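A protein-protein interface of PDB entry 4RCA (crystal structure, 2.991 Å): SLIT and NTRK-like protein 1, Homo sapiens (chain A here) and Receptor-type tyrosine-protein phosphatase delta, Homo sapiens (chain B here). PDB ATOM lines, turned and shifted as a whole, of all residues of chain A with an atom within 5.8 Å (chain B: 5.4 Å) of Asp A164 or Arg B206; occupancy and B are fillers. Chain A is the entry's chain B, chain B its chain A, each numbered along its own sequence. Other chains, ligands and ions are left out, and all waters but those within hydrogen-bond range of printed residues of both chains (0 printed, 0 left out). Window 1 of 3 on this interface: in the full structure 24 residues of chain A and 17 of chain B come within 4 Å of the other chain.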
ATOM      1  N   ARG A  91      13.437  28.246  -1.553  1.00  0.00           N
ATOM      2  CA  ARG A  91      12.948  27.226  -0.631  1.00  0.00           C
ATOM      3  C   ARG A  91      13.915  26.047  -0.506  1.00  0.00           C
ATOM      4  O   ARG A  91      14.215  25.369  -1.487  1.00  0.00           O
ATOM      5  CB  ARG A  91      11.572  26.738  -1.091  1.00  0.00           C
ATOM      6  CG  ARG A  91      10.910  25.723  -0.184  1.00  0.00           C
ATOM      7  CD  ARG A  91       9.417  25.659  -0.465  1.00  0.00           C
ATOM      8  NE  ARG A  91       8.713  24.774   0.457  1.00  0.00           N
ATOM      9  CZ  ARG A  91       7.390  24.727   0.579  1.00  0.00           C
ATOM     10  NH1 ARG A  91       6.626  25.522  -0.159  1.00  0.00           N
ATOM     11  NH2 ARG A  91       6.831  23.891   1.443  1.00  0.00           N
ATOM     12  N   TYR A 115      12.605  30.327   2.541  1.00  0.00           N
ATOM     13  CA  TYR A 115      12.023  29.204   3.262  1.00  0.00           C
ATOM     14  C   TYR A 115      13.119  28.215   3.641  1.00  0.00           C
ATOM     15  O   TYR A 115      13.842  27.738   2.774  1.00  0.00           O
ATOM     16  CB  TYR A 115      10.955  28.533   2.387  1.00  0.00           C
ATOM     17  CG  TYR A 115      10.162  27.413   3.028  1.00  0.00           C
ATOM     18  CD1 TYR A 115      10.721  26.157   3.225  1.00  0.00           C
ATOM     19  CD2 TYR A 115       8.835  27.600   3.393  1.00  0.00           C
ATOM     20  CE1 TYR A 115       9.993  25.131   3.795  1.00  0.00           C
ATOM     21  CE2 TYR A 115       8.100  26.581   3.966  1.00  0.00           C
ATOM     22  CZ  TYR A 115       8.683  25.348   4.162  1.00  0.00           C
ATOM     23  OH  TYR A 115       7.955  24.327   4.729  1.00  0.00           O
ATOM     24  N   GLN A 117      13.760  24.611   5.907  1.00  0.00           N
ATOM     25  CA  GLN A 117      13.277  23.521   6.752  1.00  0.00           C
ATOM     26  C   GLN A 117      14.415  22.602   7.174  1.00  0.00           C
ATOM     27  O   GLN A 117      15.023  21.927   6.343  1.00  0.00           O
ATOM     28  CB  GLN A 117      12.195  22.715   6.033  1.00  0.00           C
ATOM     29  CG  GLN A 117      10.796  22.949   6.575  1.00  0.00           C
ATOM     30  CD  GLN A 117       9.813  21.883   6.138  1.00  0.00           C
ATOM     31  OE1 GLN A 117       9.315  21.905   5.013  1.00  0.00           O
ATOM     32  NE2 GLN A 117       9.528  20.940   7.028  1.00  0.00           N
ATOM     33  N   ASP A 119      14.062  20.550  10.248  1.00  0.00           N
ATOM     34  CA  ASP A 119      13.531  19.766  11.358  1.00  0.00           C
ATOM     35  C   ASP A 119      14.056  18.333  11.330  1.00  0.00           C
ATOM     36  O   ASP A 119      14.451  17.835  10.279  1.00  0.00           O
ATOM     37  CB  ASP A 119      11.999  19.766  11.343  1.00  0.00           C
ATOM     38  CG  ASP A 119      11.423  19.667   9.946  1.00  0.00           C
ATOM     39  OD1 ASP A 119      11.803  20.489   9.086  1.00  0.00           O
ATOM     40  OD2 ASP A 119      10.585  18.771   9.710  1.00  0.00           O
ATOM     41  N   LEU A 140      11.433  30.015   8.971  1.00  0.00           N
ATOM     42  CA  LEU A 140      12.459  29.128   9.497  1.00  0.00           C
ATOM     43  C   LEU A 140      11.822  28.045  10.366  1.00  0.00           C
ATOM     44  O   LEU A 140      11.216  28.333  11.406  1.00  0.00           O
ATOM     45  CB  LEU A 140      13.484  29.926  10.305  1.00  0.00           C
ATOM     46  CG  LEU A 140      14.637  29.160  10.953  1.00  0.00           C
ATOM     47  CD1 LEU A 140      15.469  28.468   9.892  1.00  0.00           C
ATOM     48  CD2 LEU A 140      15.494  30.103  11.785  1.00  0.00           C
ATOM     49  N   ILE A 141      11.963  26.797   9.931  1.00  0.00           N
ATOM     50  CA  ILE A 141      11.355  25.665  10.617  1.00  0.00           C
ATOM     51  C   ILE A 141      12.429  24.743  11.190  1.00  0.00           C
ATOM     52  O   ILE A 141      13.142  24.068  10.447  1.00  0.00           O
ATOM     53  CB  ILE A 141      10.433  24.874   9.670  1.00  0.00           C
ATOM     54  CG1 ILE A 141       9.326  25.783   9.131  1.00  0.00           C
ATOM     55  CG2 ILE A 141       9.840  23.673  10.377  1.00  0.00           C
ATOM     56  CD1 ILE A 141       8.362  25.097   8.187  1.00  0.00           C
ATOM     57  N   LEU A 142      12.537  24.720  12.516  1.00  0.00           N
ATOM     58  CA  LEU A 142      13.610  23.993  13.190  1.00  0.00           C
ATOM     59  C   LEU A 142      13.101  23.017  14.247  1.00  0.00           C
ATOM     60  O   LEU A 142      13.811  22.726  15.210  1.00  0.00           O
ATOM     61  CB  LEU A 142      14.579  24.980  13.849  1.00  0.00           C
ATOM     62  CG  LEU A 142      15.224  26.049  12.967  1.00  0.00           C
ATOM     63  CD1 LEU A 142      15.980  27.055  13.820  1.00  0.00           C
ATOM     64  CD2 LEU A 142      16.148  25.410  11.945  1.00  0.00           C
ATOM     65  N   ASN A 143      11.884  22.510  14.076  1.00  0.00           N
ATOM     66  CA  ASN A 143      11.286  21.657  15.100  1.00  0.00           C
ATOM     67  C   ASN A 143      11.999  20.316  15.256  1.00  0.00           C
ATOM     68  O   ASN A 143      12.709  19.872  14.360  1.00  0.00           O
ATOM     69  CB  ASN A 143       9.800  21.421  14.810  1.00  0.00           C
ATOM     70  CG  ASN A 143       9.562  20.718  13.491  1.00  0.00           C
ATOM     71  OD1 ASN A 143       9.423  21.361  12.453  1.00  0.00           O
ATOM     72  ND2 ASN A 143       9.500  19.392  13.527  1.00  0.00           N
ATOM     73  N   HIS A 162       7.815  33.216  10.379  1.00  0.00           N
ATOM     74  CA  HIS A 162       7.411  31.925  10.919  1.00  0.00           C
ATOM     75  C   HIS A 162       8.609  31.258  11.583  1.00  0.00           C
ATOM     76  O   HIS A 162       9.560  30.891  10.914  1.00  0.00           O
ATOM     77  CB  HIS A 162       6.843  31.029   9.817  1.00  0.00           C
ATOM     78  CG  HIS A 162       6.409  29.677  10.295  1.00  0.00           C
ATOM     79  ND1 HIS A 162       5.102  29.386  10.621  1.00  0.00           N
ATOM     80  CD2 HIS A 162       7.109  28.535  10.497  1.00  0.00           C
ATOM     81  CE1 HIS A 162       5.015  28.126  11.005  1.00  0.00           C
ATOM     82  NE2 HIS A 162       6.220  27.586  10.939  1.00  0.00           N
ATOM     83  N   LEU A 163       8.567  31.113  12.902  1.00  0.00           N
ATOM     84  CA  LEU A 163       9.665  30.479  13.622  1.00  0.00           C
ATOM     85  C   LEU A 163       9.182  29.227  14.344  1.00  0.00           C
ATOM     86  O   LEU A 163       8.557  29.313  15.403  1.00  0.00           O
ATOM     87  CB  LEU A 163      10.294  31.457  14.618  1.00  0.00           C
ATOM     88  CG  LEU A 163      11.566  30.979  15.318  1.00  0.00           C
ATOM     89  CD1 LEU A 163      12.647  30.657  14.299  1.00  0.00           C
ATOM     90  CD2 LEU A 163      12.059  32.017  16.315  1.00  0.00           C
ATOM     91  N   ASP A 164       9.469  28.063  13.768  1.00  0.00           N
ATOM     92  CA  ASP A 164       9.043  26.805  14.374  1.00  0.00           C
ATOM     93  C   ASP A 164      10.186  26.180  15.171  1.00  0.00           C
ATOM     94  O   ASP A 164      11.111  25.606  14.599  1.00  0.00           O
ATOM     95  CB  ASP A 164       8.537  25.833  13.301  1.00  0.00           C
ATOM     96  CG  ASP A 164       7.683  24.715  13.878  1.00  0.00           C
ATOM     97  OD1 ASP A 164       8.098  24.093  14.879  1.00  0.00           O
ATOM     98  OD2 ASP A 164       6.589  24.460  13.330  1.00  0.00           O
ATOM     99  N   LEU A 165      10.110  26.295  16.494  1.00  0.00           N
ATOM    100  CA  LEU A 165      11.180  25.834  17.375  1.00  0.00           C
ATOM    101  C   LEU A 165      10.753  24.703  18.309  1.00  0.00           C
ATOM    102  O   LEU A 165      11.408  24.454  19.320  1.00  0.00           O
ATOM    103  CB  LEU A 165      11.712  27.000  18.213  1.00  0.00           C
ATOM    104  CG  LEU A 165      12.643  27.997  17.523  1.00  0.00           C
ATOM    105  CD1 LEU A 165      12.947  29.167  18.446  1.00  0.00           C
ATOM    106  CD2 LEU A 165      13.926  27.304  17.096  1.00  0.00           C
ATOM    107  N   ARG A 166       9.664  24.021  17.974  1.00  0.00           N
ATOM    108  CA  ARG A 166       9.148  22.955  18.830  1.00  0.00           C
ATOM    109  C   ARG A 166      10.121  21.783  18.959  1.00  0.00           C
ATOM    110  O   ARG A 166      11.011  21.611  18.134  1.00  0.00           O
ATOM    111  CB  ARG A 166       7.802  22.451  18.300  1.00  0.00           C
ATOM    112  CG  ARG A 166       6.639  23.407  18.516  1.00  0.00           C
ATOM    113  CD  ARG A 166       5.386  22.895  17.825  1.00  0.00           C
ATOM    114  NE  ARG A 166       5.554  22.856  16.374  1.00  0.00           N
ATOM    115  CZ  ARG A 166       4.737  22.222  15.540  1.00  0.00           C
ATOM    116  NH1 ARG A 166       3.688  21.558  16.008  1.00  0.00           N
ATOM    117  NH2 ARG A 166       4.972  22.246  14.236  1.00  0.00           N
ATOM    118  N   ASN A 168      12.657  20.925  21.059  1.00  0.00           N
ATOM    119  CA  ASN A 168      14.081  21.095  21.338  1.00  0.00           C
ATOM    120  C   ASN A 168      14.377  21.044  22.832  1.00  0.00           C
ATOM    121  O   ASN A 168      13.463  20.949  23.647  1.00  0.00           O
ATOM    122  CB  ASN A 168      14.588  22.415  20.755  1.00  0.00           C
ATOM    123  CG  ASN A 168      14.465  22.471  19.248  1.00  0.00           C
ATOM    124  OD1 ASN A 168      15.388  22.104  18.526  1.00  0.00           O
ATOM    125  ND2 ASN A 168      13.319  22.934  18.765  1.00  0.00           N
ATOM    126  N   GLU A 187       3.780  33.760  13.209  1.00  0.00           N
ATOM    127  CA  GLU A 187       3.610  32.413  13.740  1.00  0.00           C
ATOM    128  C   GLU A 187       4.890  31.966  14.432  1.00  0.00           C
ATOM    129  O   GLU A 187       5.933  31.852  13.796  1.00  0.00           O
ATOM    130  CB  GLU A 187       3.252  31.421  12.629  1.00  0.00           C
ATOM    131  CG  GLU A 187       1.897  31.642  11.977  1.00  0.00           C
ATOM    132  CD  GLU A 187       1.637  30.669  10.843  1.00  0.00           C
ATOM    133  OE1 GLU A 187       2.599  30.012  10.390  1.00  0.00           O
ATOM    134  OE2 GLU A 187       0.473  30.557  10.406  1.00  0.00           O
ATOM    135  N   ILE A 188       4.817  31.721  15.734  1.00  0.00           N
ATOM    136  CA  ILE A 188       5.956  31.152  16.438  1.00  0.00           C
ATOM    137  C   ILE A 188       5.500  29.935  17.239  1.00  0.00           C
ATOM    138  O   ILE A 188       4.434  29.941  17.858  1.00  0.00           O
ATOM    139  CB  ILE A 188       6.652  32.194  17.351  1.00  0.00           C
ATOM    140  CG1 ILE A 188       7.972  31.636  17.891  1.00  0.00           C
ATOM    141  CG2 ILE A 188       5.733  32.659  18.474  1.00  0.00           C
ATOM    142  CD1 ILE A 188       8.876  32.680  18.504  1.00  0.00           C
ATOM    143  N   LEU A 189       6.299  28.874  17.187  1.00  0.00           N
ATOM    144  CA  LEU A 189       5.934  27.614  17.822  1.00  0.00           C
ATOM    145  C   LEU A 189       7.031  27.157  18.775  1.00  0.00           C
ATOM    146  O   LEU A 189       8.125  26.787  18.348  1.00  0.00           O
ATOM    147  CB  LEU A 189       5.658  26.538  16.766  1.00  0.00           C
ATOM    148  CG  LEU A 189       4.615  26.868  15.690  1.00  0.00           C
ATOM    149  CD1 LEU A 189       5.252  27.553  14.486  1.00  0.00           C
ATOM    150  CD2 LEU A 189       3.862  25.620  15.259  1.00  0.00           C
ATOM    151  N   VAL B 116       2.095  29.125   7.355  1.00  0.00           N
ATOM    152  CA  VAL B 116       2.640  27.815   7.035  1.00  0.00           C
ATOM    153  C   VAL B 116       1.742  26.747   7.640  1.00  0.00           C
ATOM    154  O   VAL B 116       1.683  26.592   8.861  1.00  0.00           O
ATOM    155  CB  VAL B 116       4.074  27.639   7.561  1.00  0.00           C
ATOM    156  CG1 VAL B 116       4.683  26.356   7.015  1.00  0.00           C
ATOM    157  CG2 VAL B 116       4.927  28.840   7.184  1.00  0.00           C
ATOM    158  N   VAL B 117       1.033  26.017   6.787  1.00  0.00           N
ATOM    159  CA  VAL B 117       0.098  25.008   7.261  1.00  0.00           C
ATOM    160  C   VAL B 117       0.600  23.604   6.931  1.00  0.00           C
ATOM    161  O   VAL B 117       1.176  23.367   5.866  1.00  0.00           O
ATOM    162  CB  VAL B 117      -1.317  25.226   6.662  1.00  0.00           C
ATOM    163  CG1 VAL B 117      -1.327  24.967   5.157  1.00  0.00           C
ATOM    164  CG2 VAL B 117      -2.345  24.356   7.373  1.00  0.00           C
ATOM    165  N   GLU B 118       0.413  22.681   7.867  1.00  0.00           N
ATOM    166  CA  GLU B 118       0.740  21.285   7.627  1.00  0.00           C
ATOM    167  C   GLU B 118      -0.314  20.689   6.704  1.00  0.00           C
ATOM    168  O   GLU B 118      -1.503  20.981   6.846  1.00  0.00           O
ATOM    169  CB  GLU B 118       0.825  20.513   8.945  1.00  0.00           C
ATOM    170  CG  GLU B 118       1.907  21.036   9.879  1.00  0.00           C
ATOM    171  CD  GLU B 118       1.909  20.343  11.227  1.00  0.00           C
ATOM    172  OE1 GLU B 118       1.267  19.279  11.355  1.00  0.00           O
ATOM    173  OE2 GLU B 118       2.554  20.866  12.161  1.00  0.00           O
ATOM    174  N   ARG B 119       0.127  19.870   5.754  1.00  0.00           N
ATOM    175  CA  ARG B 119      -0.749  19.353   4.706  1.00  0.00           C
ATOM    176  C   ARG B 119      -1.956  18.601   5.273  1.00  0.00           C
ATOM    177  O   ARG B 119      -1.883  18.022   6.358  1.00  0.00           O
ATOM    178  CB  ARG B 119       0.046  18.450   3.757  1.00  0.00           C
ATOM    179  CG  ARG B 119      -0.700  18.050   2.493  1.00  0.00           C
ATOM    180  CD  ARG B 119       0.252  17.726   1.352  1.00  0.00           C
ATOM    181  NE  ARG B 119       1.175  16.646   1.688  1.00  0.00           N
ATOM    182  CZ  ARG B 119       0.884  15.353   1.588  1.00  0.00           C
ATOM    183  NH1 ARG B 119      -0.315  14.970   1.170  1.00  0.00           N
ATOM    184  NH2 ARG B 119       1.791  14.443   1.914  1.00  0.00           N
ATOM    185  N   TYR B 204       2.159  28.890   2.749  1.00  0.00           N
ATOM    186  CA  TYR B 204       3.061  27.762   2.544  1.00  0.00           C
ATOM    187  C   TYR B 204       2.413  26.479   3.052  1.00  0.00           C
ATOM    188  O   TYR B 204       1.616  26.507   3.989  1.00  0.00           O
ATOM    189  CB  TYR B 204       4.404  27.992   3.247  1.00  0.00           C
ATOM    190  CG  TYR B 204       5.259  29.093   2.648  1.00  0.00           C
ATOM    191  CD1 TYR B 204       6.057  28.854   1.536  1.00  0.00           C
ATOM    192  CD2 TYR B 204       5.284  30.365   3.208  1.00  0.00           C
ATOM    193  CE1 TYR B 204       6.847  29.854   0.990  1.00  0.00           C
ATOM    194  CE2 TYR B 204       6.071  31.370   2.670  1.00  0.00           C
ATOM    195  CZ  TYR B 204       6.849  31.110   1.563  1.00  0.00           C
ATOM    196  OH  TYR B 204       7.630  32.111   1.028  1.00  0.00           O
ATOM    197  N   VAL B 205       2.747  25.357   2.425  1.00  0.00           N
ATOM    198  CA  VAL B 205       2.232  24.062   2.858  1.00  0.00           C
ATOM    199  C   VAL B 205       3.372  23.088   3.124  1.00  0.00           C
ATOM    200  O   VAL B 205       4.168  22.789   2.233  1.00  0.00           O
ATOM    201  CB  VAL B 205       1.271  23.453   1.823  1.00  0.00           C
ATOM    202  CG1 VAL B 205       0.897  22.031   2.214  1.00  0.00           C
ATOM    203  CG2 VAL B 205       0.030  24.318   1.695  1.00  0.00           C
ATOM    204  N   ARG B 206       3.441  22.603   4.358  1.00  0.00           N
ATOM    205  CA  ARG B 206       4.494  21.687   4.771  1.00  0.00           C
ATOM    206  C   ARG B 206       3.928  20.309   5.076  1.00  0.00           C
ATOM    207  O   ARG B 206       2.716  20.098   5.018  1.00  0.00           O
ATOM    208  CB  ARG B 206       5.225  22.228   6.001  1.00  0.00           C
ATOM    209  CG  ARG B 206       4.333  22.393   7.224  1.00  0.00           C
ATOM    210  CD  ARG B 206       5.150  22.638   8.483  1.00  0.00           C
ATOM    211  NE  ARG B 206       6.002  21.499   8.809  1.00  0.00           N
ATOM    212  CZ  ARG B 206       6.763  21.421   9.897  1.00  0.00           C
ATOM    213  NH1 ARG B 206       6.779  22.418  10.771  1.00  0.00           N
ATOM    214  NH2 ARG B 206       7.507  20.344  10.112  1.00  0.00           N
ATOM    215  N   GLU B 207       4.814  19.375   5.402  1.00  0.00           N
ATOM    216  CA  GLU B 207       4.403  18.051   5.846  1.00  0.00           C
ATOM    217  C   GLU B 207       4.025  18.096   7.319  1.00  0.00           C
ATOM    218  O   GLU B 207       4.407  19.020   8.036  1.00  0.00           O
ATOM    219  CB  GLU B 207       5.516  17.028   5.614  1.00  0.00           C
ATOM    220  CG  GLU B 207       5.755  16.707   4.153  1.00  0.00           C
ATOM    221  CD  GLU B 207       4.495  16.235   3.457  1.00  0.00           C
ATOM    222  OE1 GLU B 207       3.903  15.233   3.911  1.00  0.00           O
ATOM    223  OE2 GLU B 207       4.090  16.873   2.462  1.00  0.00           O
ATOM    224  N   LEU B 208       3.271  17.099   7.769  1.00  0.00           N
ATOM    225  CA  LEU B 208       2.866  17.039   9.167  1.00  0.00           C
ATOM    226  C   LEU B 208       4.048  16.702  10.063  1.00  0.00           C
ATOM    227  O   LEU B 208       4.877  15.858   9.722  1.00  0.00           O
ATOM    228  CB  LEU B 208       1.751  16.012   9.368  1.00  0.00           C
ATOM    229  CG  LEU B 208       0.387  16.336   8.759  1.00  0.00           C
ATOM    230  CD1 LEU B 208       0.182  15.582   7.454  1.00  0.00           C
ATOM    231  CD2 LEU B 208      -0.726  16.028   9.748  1.00  0.00           C
ATOM    232  N   ARG B 209       4.123  17.372  11.207  1.00  0.00           N
ATOM    233  CA  ARG B 209       5.146  17.065  12.192  1.00  0.00           C
ATOM    234  C   ARG B 209       4.843  15.729  12.852  1.00  0.00           C
ATOM    235  O   ARG B 209       3.882  15.611  13.612  1.00  0.00           O
ATOM    236  CB  ARG B 209       5.237  18.164  13.252  1.00  0.00           C
ATOM    237  CG  ARG B 209       6.281  17.895  14.324  1.00  0.00           C
ATOM    238  CD  ARG B 209       5.924  18.586  15.629  1.00  0.00           C
ATOM    239  NE  ARG B 209       6.912  18.329  16.672  1.00  0.00           N
ATOM    240  CZ  ARG B 209       6.691  18.505  17.970  1.00  0.00           C
ATOM    241  NH1 ARG B 209       5.507  18.930  18.392  1.00  0.00           N
ATOM    242  NH2 ARG B 209       7.649  18.247  18.849  1.00  0.00           N
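The guanidinium group (NH2) of Arg B206 lies within hydrogen-bond range of the side-chain amide oxygen (OD1) of Asn A143 (3.2 Å). NH1 of Arg B206 is in salt-bridge range of OD2 of Asp A164, at 3.3 Å. OD2 of Asp A119 lies within salt-bridge range of NH2 of Arg B206 (3.5 Å). The side-chain carboxylate (OE2) of Glu B118 lies within salt-bridge range of the guanidinium group (NH2) of Arg A166 (3.5 Å). NH2 of Arg A91 lies within hydrogen-bond range of O of Val B205, at 3.0 Å. The backbone NH of Val B116 lies within hydrogen-bond range of the side-chain carboxylate of Glu A187 (3.2 Å).
N of Arg B119 sits at hydrogen-bond distance from O of Arg B206, at 2.7 Å. O of Leu A189 lies within hydrogen-bond range of N of Arg A166, at 3.2 Å. O of Arg A166 is in hydrogen-bond range of ND2 of Asn A168 (2.7 Å). The backbone NH (N) of Leu A163 is in hydrogen-bond range of the backbone carbonyl oxygen (O) of Glu A187 (2.9 Å). OE1 of Glu B118 lies within hydrogen-bond range of N of Arg B209. N of Asn A143 is in hydrogen-bond range of O of Asp A164.
Of chain B, only Arg B206 comes within 4 Å of Asp A164. Arg B206 touches just these residues of chain A: Tyr A115, Gln A117, Asp A119, Ile A141, Asn A143, Asp A164 and Arg A166. Printed residues of chain B within 4 Å of Asn A143: Arg B206 and Arg B209. Of the printed residues of chain B, Arg A91 touches Tyr B204 and Val B205. Printed residues of chain A within 4 Å of Val B205: Arg A91 (3.0 Å). Of the printed residues of chain A, Tyr B204 touches Arg A91 and Tyr A115. Leu A165 touches none of the printed residues of chain B. Arg B119 touches none of the printed residues of chain A.
Of the 10 printed residues of chain B, 6 touch a printed residue of chain A. Hydrophobic or aromatic side chains of chain B that line the printed part of chain A: Val B116 and Tyr B204. Printed residues of chain A that touch a printed residue of chain B: Arg A91, Tyr A115, Gln A117, Asp A119, Ile A141, Asn A143, His A162, Asp A164, Arg A166 and Glu A187. Along chain A the printed residues that touch a printed residue of chain B span positions 91 to 187. Among the printed residues, 15 pairs touch across the chains. Among the printed residues, Asp or Glu carboxylates within 4 Å of a Lys or Arg side-chain nitrogen of the other chain: Asp A119 with Arg B206 (3.5 Å), Asp A164 with Arg B206 (3.3 Å) and Arg A166 with Glu B118 (3.5 Å).
Arg A91 touches Tyr B204 (NH1 to CD1, 3.8 Å). Tyr A115 touches Tyr B204 (CD2 to CD1, 3.6 Å). Tyr A115 touches Arg B206 (OH to CB, 3.7 Å). NE2 of Gln A117 touches NH2 of Arg B206, at 3.7 Å. CG2 of Ile A141 touches NH1 of Arg B206, at 3.3 Å. Asn A143 touches Arg B209 (ND2 to CG, 3.6 Å). CG2 of Val B116 touches ND1 of His A162, at 3.5 Å. Arg A166 touches Arg B206. Arg A166 touches Arg B209.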
